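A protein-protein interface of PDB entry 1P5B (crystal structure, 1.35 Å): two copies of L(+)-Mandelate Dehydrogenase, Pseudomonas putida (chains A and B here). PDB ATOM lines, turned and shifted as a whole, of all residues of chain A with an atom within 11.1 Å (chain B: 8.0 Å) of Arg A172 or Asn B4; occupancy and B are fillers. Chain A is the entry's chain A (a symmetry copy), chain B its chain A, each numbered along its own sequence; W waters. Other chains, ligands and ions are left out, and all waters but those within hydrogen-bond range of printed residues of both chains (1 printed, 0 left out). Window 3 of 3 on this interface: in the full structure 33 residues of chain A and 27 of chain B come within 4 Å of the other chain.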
ATOM      1  N   LYS A  21      25.212  -2.494 -11.071  1.00  0.00           N
ATOM      2  CA  LYS A  21      24.931  -1.059 -11.119  1.00  0.00           C
ATOM      3  C   LYS A  21      25.195  -0.336  -9.800  1.00  0.00           C
ATOM      4  O   LYS A  21      25.822   0.726  -9.784  1.00  0.00           O
ATOM      5  CB  LYS A  21      23.482  -0.814 -11.545  1.00  0.00           C
ATOM      6  CG  LYS A  21      23.071   0.651 -11.472  1.00  0.00           C
ATOM      7  CD  LYS A  21      21.630   0.853 -11.904  1.00  0.00           C
ATOM      8  CE  LYS A  21      21.177   2.282 -11.648  1.00  0.00           C
ATOM      9  NZ  LYS A  21      22.023   3.274 -12.364  1.00  0.00           N
ATOM     10  N   MET A  22      24.712  -0.907  -8.703  1.00  0.00           N
ATOM     11  CA  MET A  22      24.878  -0.319  -7.376  1.00  0.00           C
ATOM     12  C   MET A  22      26.342  -0.031  -7.059  1.00  0.00           C
ATOM     13  O   MET A  22      26.679   1.021  -6.512  1.00  0.00           O
ATOM     14  CB  MET A  22      24.317  -1.266  -6.313  1.00  0.00           C
ATOM     15  CG  MET A  22      24.369  -0.724  -4.894  1.00  0.00           C
ATOM     16  SD  MET A  22      23.993  -1.987  -3.655  1.00  0.00           S
ATOM     17  CE  MET A  22      22.329  -2.450  -4.138  1.00  0.00           C
ATOM     18  N   VAL A  23      27.204  -0.982  -7.399  1.00  0.00           N
ATOM     19  CA  VAL A  23      28.629  -0.856  -7.139  1.00  0.00           C
ATOM     20  C   VAL A  23      29.273   0.154  -8.077  1.00  0.00           C
ATOM     21  O   VAL A  23      30.090   0.967  -7.649  1.00  0.00           O
ATOM     22  CB  VAL A  23      29.334  -2.223  -7.268  1.00  0.00           C
ATOM     23  CG1 VAL A  23      30.819  -2.074  -6.983  1.00  0.00           C
ATOM     24  CG2 VAL A  23      28.715  -3.216  -6.286  1.00  0.00           C
ATOM     25  N   ASP A  25      27.848   2.665  -9.425  1.00  0.00           N
ATOM     26  CA  ASP A  25      27.409   3.987  -8.986  1.00  0.00           C
ATOM     27  C   ASP A  25      28.160   4.437  -7.738  1.00  0.00           C
ATOM     28  O   ASP A  25      28.462   5.620  -7.585  1.00  0.00           O
ATOM     29  CB  ASP A  25      25.899   4.005  -8.728  1.00  0.00           C
ATOM     30  CG  ASP A  25      25.091   4.006 -10.015  1.00  0.00           C
ATOM     31  OD1 ASP A  25      25.636   4.407 -11.065  1.00  0.00           O
ATOM     32  OD2 ASP A  25      23.906   3.620  -9.972  1.00  0.00           O
ATOM     33  N   TYR A  26      28.455   3.502  -6.840  1.00  0.00           N
ATOM     34  CA  TYR A  26      29.205   3.823  -5.632  1.00  0.00           C
ATOM     35  C   TYR A  26      30.577   4.354  -6.041  1.00  0.00           C
ATOM     36  O   TYR A  26      31.082   5.326  -5.480  1.00  0.00           O
ATOM     37  CB  TYR A  26      29.386   2.566  -4.769  1.00  0.00           C
ATOM     38  CG  TYR A  26      30.561   2.636  -3.812  1.00  0.00           C
ATOM     39  CD1 TYR A  26      30.531   3.471  -2.699  1.00  0.00           C
ATOM     40  CD2 TYR A  26      31.722   1.894  -4.050  1.00  0.00           C
ATOM     41  CE1 TYR A  26      31.631   3.573  -1.842  1.00  0.00           C
ATOM     42  CE2 TYR A  26      32.825   1.989  -3.202  1.00  0.00           C
ATOM     43  CZ  TYR A  26      32.773   2.830  -2.103  1.00  0.00           C
ATOM     44  OH  TYR A  26      33.867   2.945  -1.275  1.00  0.00           O
ATOM     45  N   TYR A 164      26.719  13.914   0.334  1.00  0.00           N
ATOM     46  CA  TYR A 164      25.369  13.584  -0.097  1.00  0.00           C
ATOM     47  C   TYR A 164      25.416  13.049  -1.524  1.00  0.00           C
ATOM     48  O   TYR A 164      25.204  13.789  -2.485  1.00  0.00           O
ATOM     49  CB  TYR A 164      24.489  14.835  -0.028  1.00  0.00           C
ATOM     50  CG  TYR A 164      23.006  14.554   0.077  1.00  0.00           C
ATOM     51  CD1 TYR A 164      22.465  13.975   1.225  1.00  0.00           C
ATOM     52  CD2 TYR A 164      22.140  14.893  -0.961  1.00  0.00           C
ATOM     53  CE1 TYR A 164      21.098  13.745   1.339  1.00  0.00           C
ATOM     54  CE2 TYR A 164      20.767  14.665  -0.858  1.00  0.00           C
ATOM     55  CZ  TYR A 164      20.255  14.093   0.297  1.00  0.00           C
ATOM     56  OH  TYR A 164      18.898  13.884   0.420  1.00  0.00           O
ATOM     57  N   ARG A 165      25.716  11.759  -1.656  1.00  0.00           N
ATOM     58  CA  ARG A 165      25.794  11.115  -2.961  1.00  0.00           C
ATOM     59  C   ARG A 165      24.439  10.498  -3.262  1.00  0.00           C
ATOM     60  O   ARG A 165      24.056   9.463  -2.711  1.00  0.00           O
ATOM     61  CB  ARG A 165      26.912  10.071  -2.965  1.00  0.00           C
ATOM     62  CG  ARG A 165      28.294  10.708  -2.809  1.00  0.00           C
ATOM     63  CD  ARG A 165      29.406   9.801  -3.307  1.00  0.00           C
ATOM     64  NE  ARG A 165      29.679   8.692  -2.400  1.00  0.00           N
ATOM     65  CZ  ARG A 165      30.308   8.814  -1.236  1.00  0.00           C
ATOM     66  NH1 ARG A 165      30.734  10.002  -0.828  1.00  0.00           N
ATOM     67  NH2 ARG A 165      30.513   7.745  -0.481  1.00  0.00           N
ATOM     68  N   GLU A 166      23.715  11.154  -4.156  1.00  0.00           N
ATOM     69  CA  GLU A 166      22.367  10.740  -4.487  1.00  0.00           C
ATOM     70  C   GLU A 166      22.209   9.426  -5.243  1.00  0.00           C
ATOM     71  O   GLU A 166      21.145   8.811  -5.180  1.00  0.00           O
ATOM     72  CB  GLU A 166      21.658  11.915  -5.172  1.00  0.00           C
ATOM     73  CG  GLU A 166      21.692  13.145  -4.252  1.00  0.00           C
ATOM     74  CD  GLU A 166      21.148  14.424  -4.861  1.00  0.00           C
ATOM     75  OE1 GLU A 166      21.330  14.645  -6.074  1.00  0.00           O
ATOM     76  OE2 GLU A 166      20.560  15.228  -4.105  1.00  0.00           O
ATOM     77  N   ARG A 167      23.248   8.966  -5.937  1.00  0.00           N
ATOM     78  CA  ARG A 167      23.126   7.678  -6.618  1.00  0.00           C
ATOM     79  C   ARG A 167      22.968   6.609  -5.537  1.00  0.00           C
ATOM     80  O   ARG A 167      22.137   5.709  -5.655  1.00  0.00           O
ATOM     81  CB  ARG A 167      24.367   7.347  -7.448  1.00  0.00           C
ATOM     82  CG  ARG A 167      24.641   8.279  -8.605  1.00  0.00           C
ATOM     83  CD  ARG A 167      25.668   7.657  -9.538  1.00  0.00           C
ATOM     84  NE  ARG A 167      26.165   8.618 -10.515  1.00  0.00           N
ATOM     85  CZ  ARG A 167      26.703   8.282 -11.682  1.00  0.00           C
ATOM     86  NH1 ARG A 167      26.811   7.003 -12.024  1.00  0.00           N
ATOM     87  NH2 ARG A 167      27.135   9.226 -12.506  1.00  0.00           N
ATOM     88  N   ASP A 168      23.775   6.714  -4.485  1.00  0.00           N
ATOM     89  CA  ASP A 168      23.718   5.757  -3.384  1.00  0.00           C
ATOM     90  C   ASP A 168      22.351   5.780  -2.712  1.00  0.00           C
ATOM     91  O   ASP A 168      21.842   4.742  -2.289  1.00  0.00           O
ATOM     92  CB  ASP A 168      24.795   6.060  -2.338  1.00  0.00           C
ATOM     93  CG  ASP A 168      26.203   5.827  -2.857  1.00  0.00           C
ATOM     94  OD1 ASP A 168      26.354   5.211  -3.932  1.00  0.00           O
ATOM     95  OD2 ASP A 168      27.161   6.253  -2.175  1.00  0.00           O
ATOM     96  N   LEU A 169      21.762   6.968  -2.602  1.00  0.00           N
ATOM     97  CA  LEU A 169      20.449   7.107  -1.983  1.00  0.00           C
ATOM     98  C   LEU A 169      19.393   6.432  -2.851  1.00  0.00           C
ATOM     99  O   LEU A 169      18.509   5.743  -2.342  1.00  0.00           O
ATOM    100  CB  LEU A 169      20.115   8.589  -1.783  1.00  0.00           C
ATOM    101  CG  LEU A 169      21.014   9.302  -0.768  1.00  0.00           C
ATOM    102  CD1 LEU A 169      20.708  10.790  -0.761  1.00  0.00           C
ATOM    103  CD2 LEU A 169      20.796   8.705   0.617  1.00  0.00           C
ATOM    104  N   HIS A 170      19.488   6.624  -4.163  1.00  0.00           N
ATOM    105  CA  HIS A 170      18.545   6.005  -5.090  1.00  0.00           C
ATOM    106  C   HIS A 170      18.664   4.484  -5.068  1.00  0.00           C
ATOM    107  O   HIS A 170      17.662   3.771  -5.152  1.00  0.00           O
ATOM    108  CB  HIS A 170      18.791   6.490  -6.521  1.00  0.00           C
ATOM    109  CG  HIS A 170      18.186   7.824  -6.825  1.00  0.00           C
ATOM    110  ND1 HIS A 170      18.544   8.974  -6.157  1.00  0.00           N
ATOM    111  CD2 HIS A 170      17.252   8.190  -7.734  1.00  0.00           C
ATOM    112  CE1 HIS A 170      17.857   9.993  -6.643  1.00  0.00           C
ATOM    113  NE2 HIS A 170      17.067   9.545  -7.600  1.00  0.00           N
ATOM    114  N   ASN A 171      19.894   3.989  -4.962  1.00  0.00           N
ATOM    115  CA  ASN A 171      20.136   2.551  -4.949  1.00  0.00           C
ATOM    116  C   ASN A 171      20.070   1.935  -3.561  1.00  0.00           C
ATOM    117  O   ASN A 171      20.180   0.716  -3.423  1.00  0.00           O
ATOM    118  CB  ASN A 171      21.511   2.228  -5.549  1.00  0.00           C
ATOM    119  CG  ASN A 171      21.671   2.734  -6.966  1.00  0.00           C
ATOM    120  OD1 ASN A 171      20.728   2.724  -7.756  1.00  0.00           O
ATOM    121  ND2 ASN A 171      22.882   3.164  -7.302  1.00  0.00           N
ATOM    122  N   ARG A 172      19.884   2.764  -2.539  1.00  0.00           N
ATOM    123  CA  ARG A 172      19.848   2.269  -1.167  1.00  0.00           C
ATOM    124  C   ARG A 172      21.131   1.469  -0.949  1.00  0.00           C
ATOM    125  O   ARG A 172      21.118   0.385  -0.364  1.00  0.00           O
ATOM    126  CB  ARG A 172      18.622   1.375  -0.940  1.00  0.00           C
ATOM    127  CG  ARG A 172      17.328   2.135  -0.687  1.00  0.00           C
ATOM    128  CD  ARG A 172      16.822   2.840  -1.931  1.00  0.00           C
ATOM    129  NE  ARG A 172      15.803   3.833  -1.599  1.00  0.00           N
ATOM    130  CZ  ARG A 172      15.136   4.554  -2.494  1.00  0.00           C
ATOM    131  NH1 ARG A 172      15.364   4.395  -3.791  1.00  0.00           N
ATOM    132  NH2 ARG A 172      14.250   5.450  -2.090  1.00  0.00           N
ATOM    133  N   PHE A 173      22.238   2.024  -1.433  1.00  0.00           N
ATOM    134  CA  PHE A 173      23.540   1.380  -1.326  1.00  0.00           C
ATOM    135  C   PHE A 173      23.853   0.880   0.075  1.00  0.00           C
ATOM    136  O   PHE A 173      23.766   1.623   1.053  1.00  0.00           O
ATOM    137  CB  PHE A 173      24.652   2.333  -1.771  1.00  0.00           C
ATOM    138  CG  PHE A 173      26.020   1.710  -1.756  1.00  0.00           C
ATOM    139  CD1 PHE A 173      26.353   0.715  -2.665  1.00  0.00           C
ATOM    140  CD2 PHE A 173      26.967   2.102  -0.816  1.00  0.00           C
ATOM    141  CE1 PHE A 173      27.608   0.113  -2.640  1.00  0.00           C
ATOM    142  CE2 PHE A 173      28.228   1.506  -0.781  1.00  0.00           C
ATOM    143  CZ  PHE A 173      28.546   0.509  -1.697  1.00  0.00           C
ATOM    144  N   LYS A 174      24.224  -0.392   0.154  1.00  0.00           N
ATOM    145  CA  LYS A 174      24.575  -1.019   1.418  1.00  0.00           C
ATOM    146  C   LYS A 174      25.894  -1.754   1.226  1.00  0.00           C
ATOM    147  O   LYS A 174      26.066  -2.489   0.252  1.00  0.00           O
ATOM    148  CB  LYS A 174      23.486  -2.009   1.840  1.00  0.00           C
ATOM    149  N   ILE A 175      26.829  -1.540   2.146  1.00  0.00           N
ATOM    150  CA  ILE A 175      28.130  -2.194   2.071  1.00  0.00           C
ATOM    151  C   ILE A 175      27.930  -3.688   1.836  1.00  0.00           C
ATOM    152  O   ILE A 175      27.245  -4.358   2.610  1.00  0.00           O
ATOM    153  CB  ILE A 175      28.929  -1.992   3.376  1.00  0.00           C
ATOM    154  CG1 ILE A 175      29.199  -0.501   3.595  1.00  0.00           C
ATOM    155  CG2 ILE A 175      30.236  -2.771   3.315  1.00  0.00           C
ATOM    156  CD1 ILE A 175      29.900  -0.185   4.899  1.00  0.00           C
ATOM    157  N   PRO A 176      28.518  -4.228   0.755  1.00  0.00           N
ATOM    158  CA  PRO A 176      28.390  -5.652   0.436  1.00  0.00           C
ATOM    159  C   PRO A 176      28.531  -6.532   1.676  1.00  0.00           C
ATOM    160  O   PRO A 176      29.497  -6.411   2.431  1.00  0.00           O
ATOM    161  CB  PRO A 176      29.507  -5.871  -0.575  1.00  0.00           C
ATOM    162  CG  PRO A 176      29.493  -4.582  -1.334  1.00  0.00           C
ATOM    163  CD  PRO A 176      29.391  -3.553  -0.223  1.00  0.00           C
ATOM    164  N   PRO A 177      27.560  -7.431   1.898  1.00  0.00           N
ATOM    165  CA  PRO A 177      27.562  -8.336   3.051  1.00  0.00           C
ATOM    166  C   PRO A 177      28.820  -9.188   3.195  1.00  0.00           C
ATOM    167  O   PRO A 177      29.211  -9.532   4.312  1.00  0.00           O
ATOM    168  CB  PRO A 177      26.304  -9.176   2.831  1.00  0.00           C
ATOM    169  CG  PRO A 177      26.172  -9.199   1.341  1.00  0.00           C
ATOM    170  CD  PRO A 177      26.457  -7.763   0.980  1.00  0.00           C
ATOM    171  N   ASN B   4      11.696   8.509  -5.261  1.00  0.00           N
ATOM    172  CA  ASN B   4      12.942   9.144  -4.742  1.00  0.00           C
ATOM    173  C   ASN B   4      12.744  10.636  -4.505  1.00  0.00           C
ATOM    174  O   ASN B   4      12.568  11.407  -5.448  1.00  0.00           O
ATOM    175  CB  ASN B   4      14.094   8.933  -5.729  1.00  0.00           C
ATOM    176  CG  ASN B   4      14.425   7.468  -5.935  1.00  0.00           C
ATOM    177  OD1 ASN B   4      14.748   6.754  -4.985  1.00  0.00           O
ATOM    178  ND2 ASN B   4      14.350   7.014  -7.180  1.00  0.00           N
ATOM    179  N   LEU B   5      12.763  11.034  -3.238  1.00  0.00           N
ATOM    180  CA  LEU B   5      12.598  12.434  -2.864  1.00  0.00           C
ATOM    181  C   LEU B   5      13.772  12.824  -1.976  1.00  0.00           C
ATOM    182  O   LEU B   5      13.665  12.861  -0.750  1.00  0.00           O
ATOM    183  CB  LEU B   5      11.270  12.627  -2.128  1.00  0.00           C
ATOM    184  CG  LEU B   5      10.025  12.303  -2.964  1.00  0.00           C
ATOM    185  CD1 LEU B   5       8.776  12.400  -2.099  1.00  0.00           C
ATOM    186  CD2 LEU B   5       9.935  13.262  -4.142  1.00  0.00           C
ATOM    187  N   PHE B   6      14.898  13.126  -2.613  1.00  0.00           N
ATOM    188  CA  PHE B   6      16.113  13.470  -1.890  1.00  0.00           C
ATOM    189  C   PHE B   6      16.576  14.913  -2.035  1.00  0.00           C
ATOM    190  O   PHE B   6      17.515  15.333  -1.364  1.00  0.00           O
ATOM    191  CB  PHE B   6      17.230  12.518  -2.319  1.00  0.00           C
ATOM    192  CG  PHE B   6      16.920  11.073  -2.050  1.00  0.00           C
ATOM    193  CD1 PHE B   6      16.824  10.606  -0.743  1.00  0.00           C
ATOM    194  CD2 PHE B   6      16.703  10.185  -3.098  1.00  0.00           C
ATOM    195  CE1 PHE B   6      16.514   9.271  -0.484  1.00  0.00           C
ATOM    196  CE2 PHE B   6      16.394   8.847  -2.850  1.00  0.00           C
ATOM    197  CZ  PHE B   6      16.299   8.392  -1.540  1.00  0.00           C
ATOM    198  N   ASN B   7      15.925  15.668  -2.913  1.00  0.00           N
ATOM    199  CA  ASN B   7      16.277  17.068  -3.116  1.00  0.00           C
ATOM    200  C   ASN B   7      15.091  17.818  -3.710  1.00  0.00           C
ATOM    201  O   ASN B   7      14.042  17.229  -3.961  1.00  0.00           O
ATOM    202  CB  ASN B   7      17.504  17.195  -4.029  1.00  0.00           C
ATOM    203  CG  ASN B   7      17.295  16.561  -5.385  1.00  0.00           C
ATOM    204  OD1 ASN B   7      16.254  16.737  -6.011  1.00  0.00           O
ATOM    205  ND2 ASN B   7      18.301  15.829  -5.857  1.00  0.00           N
ATOM    206  N   GLU B   9      14.725  19.166  -6.731  1.00  0.00           N
ATOM    207  CA  GLU B   9      14.417  18.729  -8.092  1.00  0.00           C
ATOM    208  C   GLU B   9      13.493  17.509  -8.089  1.00  0.00           C
ATOM    209  O   GLU B   9      12.620  17.388  -8.944  1.00  0.00           O
ATOM    210  CB  GLU B   9      15.707  18.396  -8.856  1.00  0.00           C
ATOM    211  CG  GLU B   9      15.481  17.726 -10.214  1.00  0.00           C
ATOM    212  CD  GLU B   9      14.966  18.672 -11.290  1.00  0.00           C
ATOM    213  OE1 GLU B   9      14.466  19.766 -10.961  1.00  0.00           O
ATOM    214  OE2 GLU B   9      15.054  18.310 -12.481  1.00  0.00           O
ATOM    215  N   ASP B  10      13.689  16.602  -7.134  1.00  0.00           N
ATOM    216  CA  ASP B  10      12.838  15.420  -7.057  1.00  0.00           C
ATOM    217  C   ASP B  10      11.394  15.836  -6.801  1.00  0.00           C
ATOM    218  O   ASP B  10      10.461  15.211  -7.309  1.00  0.00           O
ATOM    219  CB  ASP B  10      13.313  14.466  -5.958  1.00  0.00           C
ATOM    220  CG  ASP B  10      14.636  13.804  -6.292  1.00  0.00           C
ATOM    221  OD1 ASP B  10      14.932  13.627  -7.491  1.00  0.00           O
ATOM    222  OD2 ASP B  10      15.373  13.446  -5.352  1.00  0.00           O
ATOM    223  N   TYR B  11      11.206  16.891  -6.011  1.00  0.00           N
ATOM    224  CA  TYR B  11       9.855  17.360  -5.746  1.00  0.00           C
ATOM    225  C   TYR B  11       9.294  18.071  -6.969  1.00  0.00           C
ATOM    226  O   TYR B  11       8.093  18.005  -7.219  1.00  0.00           O
ATOM    227  CB  TYR B  11       9.812  18.267  -4.512  1.00  0.00           C
ATOM    228  CG  TYR B  11       9.835  17.479  -3.221  1.00  0.00           C
ATOM    229  CD1 TYR B  11      11.037  17.009  -2.688  1.00  0.00           C
ATOM    230  CD2 TYR B  11       8.648  17.133  -2.574  1.00  0.00           C
ATOM    231  CE1 TYR B  11      11.057  16.211  -1.547  1.00  0.00           C
ATOM    232  CE2 TYR B  11       8.656  16.334  -1.432  1.00  0.00           C
ATOM    233  CZ  TYR B  11       9.864  15.876  -0.928  1.00  0.00           C
ATOM    234  OH  TYR B  11       9.884  15.064   0.179  1.00  0.00           O
ATOM    235  N   LYS B  13       9.875  17.223 -10.014  1.00  0.00           N
ATOM    236  CA  LYS B  13       9.465  16.123 -10.878  1.00  0.00           C
ATOM    237  C   LYS B  13       8.121  15.546 -10.448  1.00  0.00           C
ATOM    238  O   LYS B  13       7.261  15.269 -11.286  1.00  0.00           O
ATOM    239  CB  LYS B  13      10.534  15.023 -10.881  1.00  0.00           C
ATOM    240  CG  LYS B  13      11.836  15.447 -11.545  1.00  0.00           C
ATOM    241  CD  LYS B  13      12.906  14.366 -11.457  1.00  0.00           C
ATOM    242  CE  LYS B  13      14.197  14.828 -12.124  1.00  0.00           C
ATOM    243  NZ  LYS B  13      15.291  13.827 -11.995  1.00  0.00           N
ATOM    244  N   LEU B  14       7.935  15.367  -9.143  1.00  0.00           N
ATOM    245  CA  LEU B  14       6.682  14.824  -8.635  1.00  0.00           C
ATOM    246  C   LEU B  14       5.549  15.830  -8.829  1.00  0.00           C
ATOM    247  O   LEU B  14       4.428  15.454  -9.177  1.00  0.00           O
ATOM    248  CB  LEU B  14       6.827  14.453  -7.154  1.00  0.00           C
ATOM    249  CG  LEU B  14       5.635  13.746  -6.499  1.00  0.00           C
ATOM    250  CD1 LEU B  14       5.235  12.531  -7.325  1.00  0.00           C
ATOM    251  CD2 LEU B  14       6.001  13.330  -5.084  1.00  0.00           C
ATOM    252  N   LEU B 328      14.897  18.834   4.172  1.00  0.00           N
ATOM    253  CA  LEU B 328      16.014  18.525   3.285  1.00  0.00           C
ATOM    254  C   LEU B 328      16.943  19.725   3.135  1.00  0.00           C
ATOM    255  O   LEU B 328      18.165  19.581   3.187  1.00  0.00           O
ATOM    256  CB  LEU B 328      15.504  18.105   1.906  1.00  0.00           C
ATOM    257  CG  LEU B 328      14.879  16.714   1.791  1.00  0.00           C
ATOM    258  CD1 LEU B 328      14.273  16.547   0.407  1.00  0.00           C
ATOM    259  CD2 LEU B 328      15.937  15.644   2.046  1.00  0.00           C
HETATM  260  O   HOH W   1      15.014  11.265  -9.016  1.00  0.00           O
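NH1 of Arg A172 sits at hydrogen-bond distance from OD1 of Asn B4 (2.7 Å).
OH of Tyr A164 lies within hydrogen-bond range of O of Phe B6 (2.7 Å).
The side-chain carboxylate of Glu A166 sits at hydrogen-bond distance from the side-chain amide nitrogen of Asn B7 (2.9 Å).
No position is printed for both chains.
Of the printed residues of chain B, Arg A172 touches Asn B4 and Phe B6.
No residue of chain A comes within 4 Å of Leu B5.
No residue of chain A comes within 4 Å of Asp B10.
Of the printed residues of chain B, Tyr A164 touches Phe B6 (2.7 Å) and Leu B328 (3.8 Å).
Of the printed residues of chain B, His A170 touches Asn B4 and Phe B6.
Printed residues of chain A within 4 Å of Phe B6: Tyr A164, Leu A169, His A170 and Arg A172.
Of the printed residues of chain B, Glu A166 touches Asn B7.
Printed residues of chain A within 4 Å of Leu B328: Tyr A164 (3.8 Å).
Lys A21 touches none of the printed residues of chain B.
The nearest residue of chain B that does not touch Arg A172 is Leu B5 (5.9 Å).
The nearest residue of chain A that does not touch Asn B4 is Leu A169 (4.7 Å).
The side-chain carboxylate (OD2) of Asp B10 lies within hydrogen-bond range of the backbone NH (N) of Phe B6, at 2.8 Å.
OD1 of Asn B7 sits at hydrogen-bond distance from N of Glu B9 (3.0 Å).
OD1 of Asn B7 lies within hydrogen-bond range of N of Asp B10, at 2.8 Å.
A ring nitrogen (ND1) of His A170 is in hydrogen-bond range of the backbone carbonyl oxygen of Glu A166 (2.8 Å).
O of Leu A169 sits close to NE of Arg A172 (3.4 Å).
The backbone carbonyl oxygen (O) of His A170 lies within hydrogen-bond range of the guanidinium group (NH1) of Arg A172, 2.7 Å away.
Leu B328 touches Tyr A164 (CD2 to OH, 3.8 Å).
CZ of Phe B6 touches O of Leu A169 (3.5 Å).
ND2 of Asn B4 touches CD2 of His A170 (3.2 Å).
His A170 touches Phe B6 (CE1 to CD2, 3.7 Å).
Phe B6 touches Arg A172.
Printed residues of chain A that touch a printed residue of chain B: Tyr A164, Glu A166, Leu A169, His A170 and Arg A172.
Hydrophobic or aromatic side chains of chain A that line the printed part of chain B: Tyr A164, Leu A169 and His A170.
Hydrophobic or aromatic side chains of chain B within 4 Å of the printed part of chain A: Phe B6 and Leu B328.
Among the printed residues, no Asp or Glu carboxylate lies within 4 Å of a Lys or Arg side-chain nitrogen of the other chain.
Water W1 lies within hydrogen-bond range of the side-chain carboxylate (OD1) of Asp B10 (2.8 Å) and a ring nitrogen (NE2) of His A170 (3.0 Å).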
